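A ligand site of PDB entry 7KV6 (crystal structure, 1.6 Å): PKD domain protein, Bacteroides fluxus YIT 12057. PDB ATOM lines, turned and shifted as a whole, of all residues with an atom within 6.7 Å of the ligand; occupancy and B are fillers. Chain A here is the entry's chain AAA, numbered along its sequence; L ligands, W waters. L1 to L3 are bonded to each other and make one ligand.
CG1 of Val 149 touches O4 of LG2 L2 (3.5 Å). CE3 of Trp 164 touches C6 of LG3 L3 (3.8 Å). Trp 165 touches the ligand. CH2 of Trp 282 touches O4 of LIG L1, at 3.7 Å. Hydrophobic or aromatic side chains that line the ligand: Val 149, Trp 164, Trp 165, Tyr 201 and Trp 282. Of the 19 residues printed, 8 come within 4 Å of the ligand.
The side-chain carboxylate (OD2) of Asp 221 lies within hydrogen-bond range of an oxygen (O6) of LIG L1 (2.7 Å). NZ of Lys 172 lies within hydrogen-bond range of O6 of LIG L1, at 2.9 Å. An oxygen (O1) of LG3 L3 is in hydrogen-bond range of the side-chain amide nitrogen of Asn 280. O6 of LIG L1 sits close to OH of Tyr 201 (3.4 Å).
Water W5 lies within hydrogen-bond range of an oxygen (O5) of LG2 L2 (2.6 Å), the side-chain carboxylate (OE2) of Glu 277 (2.6 Å) and the side-chain amide nitrogen (ND2) of Asn 203 (3.5 Å). Water W3 lies within hydrogen-bond range of an oxygen (O4) of LIG L1, the side-chain carboxylate of Asp 221 and the side-chain amide nitrogen of Asn 203. Water W9 lies within hydrogen-bond range of the side-chain carboxylate (OD2) of Asp 221 (2.8 Å), an oxygen (O6) of LIG L1 (3.1 Å), a ring nitrogen (NE2) of His 251 (3.2 Å) and the backbone carbonyl oxygen (O) of Thr 202 (3.3 Å). Water W6 lies within hydrogen-bond range of the backbone carbonyl oxygen of Trp 164 (2.7 Å) and an oxygen (O2) of LG2 L2 (3.2 Å). Water W2 lies within hydrogen-bond range of NZ of Lys 172 (2.8 Å), O of Ala 219 (3.2 Å) and O1 of LIG L1 (3.3 Å). Water W8 bridges O of Ala 219 (2.7 Å) and NZ of Lys 172 (3.3 Å).
The side-chain amino group (NZ) of Lys 172 is in hydrogen-bond range of the side-chain hydroxyl (OH) of Tyr 201 (3.0 Å). O of Ala 219 lies within hydrogen-bond range of NZ of Lys 172, at 3.3 Å. The backbone carbonyl oxygen (O) of Ala 219 sits at hydrogen-bond distance from the side-chain hydroxyl (OH) of Tyr 201 (3.4 Å). OH of Tyr 201 lies within hydrogen-bond range of O of Gly 220 (2.7 Å). The backbone NH (N) of Val 149 lies within hydrogen-bond range of the backbone carbonyl oxygen (O) of Trp 165 (2.9 Å). The backbone NH of Trp 164 is in hydrogen-bond range of the backbone carbonyl oxygen of Val 149, at 3.1 Å.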
ATOM      1  N   PHE A 147     -14.507 -13.681  15.425  1.00  0.00           N
ATOM      2  CA  PHE A 147     -13.109 -14.077  15.689  1.00  0.00           C
ATOM      3  C   PHE A 147     -12.783 -13.477  17.040  1.00  0.00           C
ATOM      4  O   PHE A 147     -13.246 -12.352  17.321  1.00  0.00           O
ATOM      5  CB  PHE A 147     -12.239 -13.555  14.543  1.00  0.00           C
ATOM      6  CG  PHE A 147     -10.745 -13.760  14.667  1.00  0.00           C
ATOM      7  CD1 PHE A 147     -10.233 -14.978  15.052  1.00  0.00           C
ATOM      8  CD2 PHE A 147      -9.870 -12.740  14.335  1.00  0.00           C
ATOM      9  CE1 PHE A 147      -8.852 -15.162  15.109  1.00  0.00           C
ATOM     10  CE2 PHE A 147      -8.502 -12.917  14.426  1.00  0.00           C
ATOM     11  CZ  PHE A 147      -8.003 -14.130  14.832  1.00  0.00           C
ATOM     12  N   VAL A 149     -10.298 -14.023  21.037  1.00  0.00           N
ATOM     13  CA  VAL A 149      -9.304 -14.743  21.849  1.00  0.00           C
ATOM     14  C   VAL A 149      -9.612 -14.547  23.338  1.00  0.00           C
ATOM     15  O   VAL A 149     -10.138 -13.525  23.722  1.00  0.00           O
ATOM     16  CB  VAL A 149      -7.886 -14.279  21.465  1.00  0.00           C
ATOM     17  CG1 VAL A 149      -7.594 -12.877  21.895  1.00  0.00           C
ATOM     18  CG2 VAL A 149      -6.848 -15.232  22.013  1.00  0.00           C
ATOM     19  N   GLY A 150      -9.343 -15.566  24.097  1.00  0.00           N
ATOM     20  CA  GLY A 150      -9.593 -15.545  25.557  1.00  0.00           C
ATOM     21  C   GLY A 150      -8.890 -16.725  26.185  1.00  0.00           C
ATOM     22  O   GLY A 150      -8.287 -17.529  25.491  1.00  0.00           O
ATOM     23  N   ASN A 155      -7.304 -23.560  30.615  1.00  0.00           N
ATOM     24  CA  ASN A 155      -6.803 -22.411  31.408  1.00  0.00           C
ATOM     25  C   ASN A 155      -7.695 -22.266  32.644  1.00  0.00           C
ATOM     26  O   ASN A 155      -8.920 -22.271  32.527  1.00  0.00           O
ATOM     27  CB  ASN A 155      -6.817 -21.164  30.517  1.00  0.00           C
ATOM     28  CG  ASN A 155      -6.171 -19.930  31.112  1.00  0.00           C
ATOM     29  OD1 ASN A 155      -6.410 -19.614  32.275  1.00  0.00           O
ATOM     30  ND2 ASN A 155      -5.452 -19.168  30.299  1.00  0.00           N
ATOM     31  N   ASP A 157      -8.692 -19.689  34.002  1.00  0.00           N
ATOM     32  CA  ASP A 157      -9.521 -18.472  33.817  1.00  0.00           C
ATOM     33  C   ASP A 157     -10.586 -18.707  32.738  1.00  0.00           C
ATOM     34  O   ASP A 157     -11.294 -17.712  32.405  1.00  0.00           O
ATOM     35  CB  ASP A 157      -8.635 -17.272  33.507  1.00  0.00           C
ATOM     36  CG  ASP A 157      -7.698 -16.911  34.636  1.00  0.00           C
ATOM     37  OD1 ASP A 157      -8.101 -17.110  35.788  1.00  0.00           O
ATOM     38  OD2 ASP A 157      -6.544 -16.532  34.359  1.00  0.00           O
ATOM     39  N   TRP A 164     -10.665 -11.762  26.239  1.00  0.00           N
ATOM     40  CA  TRP A 164      -9.543 -10.821  26.089  1.00  0.00           C
ATOM     41  C   TRP A 164      -9.835  -9.853  24.955  1.00  0.00           C
ATOM     42  O   TRP A 164      -9.476  -8.674  25.075  1.00  0.00           O
ATOM     43  CB  TRP A 164      -8.228 -11.540  25.856  1.00  0.00           C
ATOM     44  CG  TRP A 164      -7.807 -12.390  27.002  1.00  0.00           C
ATOM     45  CD1 TRP A 164      -8.124 -12.220  28.323  1.00  0.00           C
ATOM     46  CD2 TRP A 164      -6.982 -13.550  26.944  1.00  0.00           C
ATOM     47  NE1 TRP A 164      -7.551 -13.202  29.084  1.00  0.00           N
ATOM     48  CE2 TRP A 164      -6.831 -14.032  28.268  1.00  0.00           C
ATOM     49  CE3 TRP A 164      -6.337 -14.226  25.906  1.00  0.00           C
ATOM     50  CZ2 TRP A 164      -6.061 -15.149  28.563  1.00  0.00           C
ATOM     51  CZ3 TRP A 164      -5.577 -15.315  26.201  1.00  0.00           C
ATOM     52  CH2 TRP A 164      -5.449 -15.780  27.512  1.00  0.00           C
ATOM     53  N   TRP A 165     -10.389 -10.343  23.834  1.00  0.00           N
ATOM     54  CA  TRP A 165     -10.601  -9.516  22.624  1.00  0.00           C
ATOM     55  C   TRP A 165     -11.606 -10.236  21.751  1.00  0.00           C
ATOM     56  O   TRP A 165     -11.434 -11.424  21.459  1.00  0.00           O
ATOM     57  CB  TRP A 165      -9.322  -9.231  21.876  1.00  0.00           C
ATOM     58  CG  TRP A 165      -9.552  -8.582  20.548  1.00  0.00           C
ATOM     59  CD1 TRP A 165      -9.820  -7.269  20.301  1.00  0.00           C
ATOM     60  CD2 TRP A 165      -9.611  -9.252  19.274  1.00  0.00           C
ATOM     61  NE1 TRP A 165      -9.964  -7.048  18.956  1.00  0.00           N
ATOM     62  CE2 TRP A 165      -9.825  -8.254  18.302  1.00  0.00           C
ATOM     63  CE3 TRP A 165      -9.413 -10.572  18.844  1.00  0.00           C
ATOM     64  CZ2 TRP A 165      -9.917  -8.555  16.952  1.00  0.00           C
ATOM     65  CZ3 TRP A 165      -9.466 -10.857  17.505  1.00  0.00           C
ATOM     66  CH2 TRP A 165      -9.744  -9.864  16.578  1.00  0.00           C
ATOM     67  N   LYS A 172     -11.155  -7.462  10.831  1.00  0.00           N
ATOM     68  CA  LYS A 172      -9.980  -8.041  10.180  1.00  0.00           C
ATOM     69  C   LYS A 172     -10.161  -8.005   8.659  1.00  0.00           C
ATOM     70  O   LYS A 172      -9.600  -8.829   7.963  1.00  0.00           O
ATOM     71  CB  LYS A 172      -9.694  -9.465  10.708  1.00  0.00           C
ATOM     72  CG  LYS A 172      -9.301  -9.495  12.158  1.00  0.00           C
ATOM     73  CD  LYS A 172      -8.012  -8.748  12.456  1.00  0.00           C
ATOM     74  CE  LYS A 172      -7.571  -8.872  13.889  1.00  0.00           C
ATOM     75  NZ  LYS A 172      -6.259  -8.239  14.138  1.00  0.00           N
ATOM     76  N   TYR A 201      -3.799 -16.000   8.085  1.00  0.00           N
ATOM     77  CA  TYR A 201      -3.565 -14.991   9.133  1.00  0.00           C
ATOM     78  C   TYR A 201      -3.077 -15.675  10.410  1.00  0.00           C
ATOM     79  O   TYR A 201      -3.523 -16.797  10.758  1.00  0.00           O
ATOM     80  CB  TYR A 201      -4.849 -14.194   9.323  1.00  0.00           C
ATOM     81  CG  TYR A 201      -4.716 -12.928  10.120  1.00  0.00           C
ATOM     82  CD1 TYR A 201      -3.783 -11.960   9.759  1.00  0.00           C
ATOM     83  CD2 TYR A 201      -5.480 -12.703  11.254  1.00  0.00           C
ATOM     84  CE1 TYR A 201      -3.649 -10.791  10.473  1.00  0.00           C
ATOM     85  CE2 TYR A 201      -5.331 -11.539  12.007  1.00  0.00           C
ATOM     86  CZ  TYR A 201      -4.430 -10.566  11.578  1.00  0.00           C
ATOM     87  OH  TYR A 201      -4.283  -9.400  12.271  1.00  0.00           O
ATOM     88  N   THR A 202      -2.126 -15.034  11.107  1.00  0.00           N
ATOM     89  CA  THR A 202      -1.562 -15.640  12.334  1.00  0.00           C
ATOM     90  C   THR A 202      -0.816 -14.527  13.083  1.00  0.00           C
ATOM     91  O   THR A 202      -0.868 -13.344  12.628  1.00  0.00           O
ATOM     92  CB  THR A 202      -0.682 -16.854  12.034  1.00  0.00           C
ATOM     93  OG1 THR A 202      -0.516 -17.554  13.266  1.00  0.00           O
ATOM     94  CG2 THR A 202       0.665 -16.505  11.402  1.00  0.00           C
ATOM     95  N   ASN A 203      -0.260 -14.882  14.232  1.00  0.00           N
ATOM     96  CA  ASN A 203       0.485 -13.896  15.046  1.00  0.00           C
ATOM     97  C   ASN A 203       1.925 -14.341  15.031  1.00  0.00           C
ATOM     98  O   ASN A 203       2.260 -15.252  14.326  1.00  0.00           O
ATOM     99  CB  ASN A 203      -0.201 -13.720  16.409  1.00  0.00           C
ATOM    100  CG  ASN A 203      -0.300 -15.006  17.193  1.00  0.00           C
ATOM    101  OD1 ASN A 203       0.322 -16.003  16.834  1.00  0.00           O
ATOM    102  ND2 ASN A 203      -1.041 -14.965  18.291  1.00  0.00           N
ATOM    103  N   ALA A 219      -4.284  -4.778   9.391  1.00  0.00           N
ATOM    104  CA  ALA A 219      -4.868  -5.208  10.678  1.00  0.00           C
ATOM    105  C   ALA A 219      -3.782  -5.584  11.696  1.00  0.00           C
ATOM    106  O   ALA A 219      -4.168  -6.064  12.773  1.00  0.00           O
ATOM    107  CB  ALA A 219      -5.783  -6.383  10.436  1.00  0.00           C
ATOM    108  N   GLY A 220      -2.514  -5.595  11.326  1.00  0.00           N
ATOM    109  CA  GLY A 220      -1.445  -6.015  12.245  1.00  0.00           C
ATOM    110  C   GLY A 220      -1.336  -7.526  12.288  1.00  0.00           C
ATOM    111  O   GLY A 220      -2.015  -8.197  11.465  1.00  0.00           O
ATOM    112  N   ASP A 221      -0.522  -8.048  13.202  1.00  0.00           N
ATOM    113  CA  ASP A 221      -0.087  -9.464  13.201  1.00  0.00           C
ATOM    114  C   ASP A 221       0.467  -9.767  11.820  1.00  0.00           C
ATOM    115  O   ASP A 221       1.157  -8.915  11.253  1.00  0.00           O
ATOM    116  CB  ASP A 221      -1.251 -10.376  13.644  1.00  0.00           C
ATOM    117  CG  ASP A 221      -1.438 -10.446  15.153  1.00  0.00           C
ATOM    118  OD1 ASP A 221      -0.545  -9.923  15.874  1.00  0.00           O
ATOM    119  OD2 ASP A 221      -2.464 -11.056  15.586  1.00  0.00           O
ATOM    120  N   HIS A 251      -6.972 -19.073  10.214  1.00  0.00           N
ATOM    121  CA  HIS A 251      -6.177 -18.496  11.315  1.00  0.00           C
ATOM    122  C   HIS A 251      -5.346 -19.637  11.869  1.00  0.00           C
ATOM    123  O   HIS A 251      -5.930 -20.650  12.278  1.00  0.00           O
ATOM    124  CB  HIS A 251      -7.078 -17.829  12.336  1.00  0.00           C
ATOM    125  CG  HIS A 251      -6.277 -17.301  13.473  1.00  0.00           C
ATOM    126  ND1 HIS A 251      -6.299 -17.893  14.736  1.00  0.00           N
ATOM    127  CD2 HIS A 251      -5.355 -16.327  13.500  1.00  0.00           C
ATOM    128  CE1 HIS A 251      -5.492 -17.172  15.525  1.00  0.00           C
ATOM    129  NE2 HIS A 251      -4.920 -16.219  14.787  1.00  0.00           N
ATOM    130  N   GLU A 277       0.641 -20.948  21.827  1.00  0.00           N
ATOM    131  CA  GLU A 277       0.556 -20.040  23.001  1.00  0.00           C
ATOM    132  C   GLU A 277      -0.258 -20.725  24.099  1.00  0.00           C
ATOM    133  O   GLU A 277      -1.524 -20.728  24.039  1.00  0.00           O
ATOM    134  CB  GLU A 277      -0.074 -18.705  22.653  1.00  0.00           C
ATOM    135  CG  GLU A 277       0.814 -17.923  21.654  1.00  0.00           C
ATOM    136  CD  GLU A 277       0.179 -16.671  21.087  1.00  0.00           C
ATOM    137  OE1 GLU A 277      -0.966 -16.767  20.519  1.00  0.00           O
ATOM    138  OE2 GLU A 277       0.736 -15.570  21.277  1.00  0.00           O
ATOM    139  N   SER A 278       0.456 -21.342  25.024  1.00  0.00           N
ATOM    140  CA  SER A 278      -0.155 -22.213  26.046  1.00  0.00           C
ATOM    141  C   SER A 278      -1.250 -21.477  26.794  1.00  0.00           C
ATOM    142  O   SER A 278      -1.010 -20.374  27.338  1.00  0.00           O
ATOM    143  CB  SER A 278       0.906 -22.719  26.990  1.00  0.00           C
ATOM    144  OG  SER A 278       0.301 -23.451  28.025  1.00  0.00           O
ATOM    145  N   ASN A 280      -3.991 -20.090  25.604  1.00  0.00           N
ATOM    146  CA  ASN A 280      -4.757 -19.129  24.808  1.00  0.00           C
ATOM    147  C   ASN A 280      -5.774 -19.915  23.968  1.00  0.00           C
ATOM    148  O   ASN A 280      -5.393 -20.891  23.283  1.00  0.00           O
ATOM    149  CB  ASN A 280      -3.823 -18.275  23.944  1.00  0.00           C
ATOM    150  CG  ASN A 280      -3.049 -17.282  24.809  1.00  0.00           C
ATOM    151  OD1 ASN A 280      -2.850 -17.529  26.008  1.00  0.00           O
ATOM    152  ND2 ASN A 280      -2.633 -16.193  24.198  1.00  0.00           N
ATOM    153  N   TRP A 282      -8.967 -19.579  20.981  1.00  0.00           N
ATOM    154  CA  TRP A 282      -9.521 -18.795  19.857  1.00  0.00           C
ATOM    155  C   TRP A 282     -10.951 -19.232  19.579  1.00  0.00           C
ATOM    156  O   TRP A 282     -11.292 -20.416  19.770  1.00  0.00           O
ATOM    157  CB  TRP A 282      -8.648 -18.957  18.619  1.00  0.00           C
ATOM    158  CG  TRP A 282      -7.251 -18.442  18.830  1.00  0.00           C
ATOM    159  CD1 TRP A 282      -6.139 -19.179  19.171  1.00  0.00           C
ATOM    160  CD2 TRP A 282      -6.795 -17.106  18.628  1.00  0.00           C
ATOM    161  NE1 TRP A 282      -5.029 -18.380  19.193  1.00  0.00           N
ATOM    162  CE2 TRP A 282      -5.404 -17.098  18.902  1.00  0.00           C
ATOM    163  CE3 TRP A 282      -7.409 -15.922  18.235  1.00  0.00           C
ATOM    164  CZ2 TRP A 282      -4.636 -15.930  18.769  1.00  0.00           C
ATOM    165  CZ3 TRP A 282      -6.657 -14.771  18.158  1.00  0.00           C
ATOM    166  CH2 TRP A 282      -5.287 -14.791  18.410  1.00  0.00           C
HETATM  167  C1  LIG L   1      -6.060  -7.854  19.290  1.00  0.00           C
HETATM  168  C2  LIG L   1      -5.362  -9.009  19.882  1.00  0.00           C
HETATM  169  C3  LIG L   1      -5.598 -10.203  18.952  1.00  0.00           C
HETATM  170  C4  LIG L   1      -5.256  -9.918  17.503  1.00  0.00           C
HETATM  171  C5  LIG L   1      -5.640 -11.044  16.588  1.00  0.00           C
HETATM  172  C6  LIG L   1      -5.593  -7.691  17.826  1.00  0.00           C
HETATM  173  O1  LIG L   1      -6.247  -6.582  17.322  1.00  0.00           O
HETATM  174  O2  LIG L   1      -5.786  -6.586  19.964  1.00  0.00           O
HETATM  175  O3  LIG L   1      -5.844  -9.144  21.154  1.00  0.00           O
HETATM  176  O4  LIG L   1      -4.704 -11.228  19.364  1.00  0.00           O
HETATM  177  O5  LIG L   1      -6.013  -8.831  17.032  1.00  0.00           O
HETATM  178  O6  LIG L   1      -5.155 -10.716  15.283  1.00  0.00           O
HETATM  179  C1  LG2 L   2      -5.366  -9.197  23.531  1.00  0.00           C
HETATM  180  C2  LG2 L   2      -4.416  -9.684  24.607  1.00  0.00           C
HETATM  181  C3  LG2 L   2      -4.086 -11.126  24.413  1.00  0.00           C
HETATM  182  C4  LG2 L   2      -3.699 -11.440  22.929  1.00  0.00           C
HETATM  183  C5  LG2 L   2      -3.594 -12.918  22.645  1.00  0.00           C
HETATM  184  C6  LG2 L   2      -4.902  -9.561  22.121  1.00  0.00           C
HETATM  185  O1  LG2 L   2      -5.456  -7.794  23.630  1.00  0.00           O
HETATM  186  O2  LG2 L   2      -5.044  -9.363  25.864  1.00  0.00           O
HETATM  187  O3  LG2 L   2      -2.984 -11.537  25.066  1.00  0.00           O
HETATM  188  O4  LG2 L   2      -4.710 -10.948  22.056  1.00  0.00           O
HETATM  189  O5  LG2 L   2      -3.086 -13.230  21.325  1.00  0.00           O
HETATM  190  C1  LG3 L   3      -1.953 -12.879  26.725  1.00  0.00           C
HETATM  191  C2  LG3 L   3      -2.150 -13.619  28.049  1.00  0.00           C
HETATM  192  C3  LG3 L   3      -2.610 -12.690  29.129  1.00  0.00           C
HETATM  193  C4  LG3 L   3      -3.763 -11.801  28.707  1.00  0.00           C
HETATM  194  C5  LG3 L   3      -3.758 -10.566  29.605  1.00  0.00           C
HETATM  195  C6  LG3 L   3      -3.199 -12.207  26.348  1.00  0.00           C
HETATM  196  O1  LG3 L   3      -1.462 -13.760  25.727  1.00  0.00           O
HETATM  197  O2  LG3 L   3      -0.904 -14.217  28.427  1.00  0.00           O
HETATM  198  O3  LG3 L   3      -2.904 -13.501  30.288  1.00  0.00           O
HETATM  199  O4  LG3 L   3      -3.642 -11.272  27.331  1.00  0.00           O
HETATM  200  O5  LG3 L   3      -5.100 -10.171  29.703  1.00  0.00           O
HETATM  201  O   HOH W   1      -7.921  -8.653  29.231  1.00  0.00           O
HETATM  202  O   HOH W   2      -6.952  -5.496  14.316  1.00  0.00           O
HETATM  203  O   HOH W   3      -2.360 -12.110  18.256  1.00  0.00           O
HETATM  204  O   HOH W   4      -3.115 -16.041  21.705  1.00  0.00           O
HETATM  205  O   HOH W   5      -0.522 -13.296  21.305  1.00  0.00           O
HETATM  206  O   HOH W   6      -7.617  -7.826  26.848  1.00  0.00           O
HETATM  207  O   HOH W   7       0.102 -12.438  23.977  1.00  0.00           O
HETATM  208  O   HOH W   8      -3.390  -7.006  15.196  1.00  0.00           O
HETATM  209  O   HOH W   9      -3.614 -13.345  14.502  1.00  0.00           O
HETATM  210  O   HOH W  10      -0.231 -16.386  27.057  1.00  0.00           O
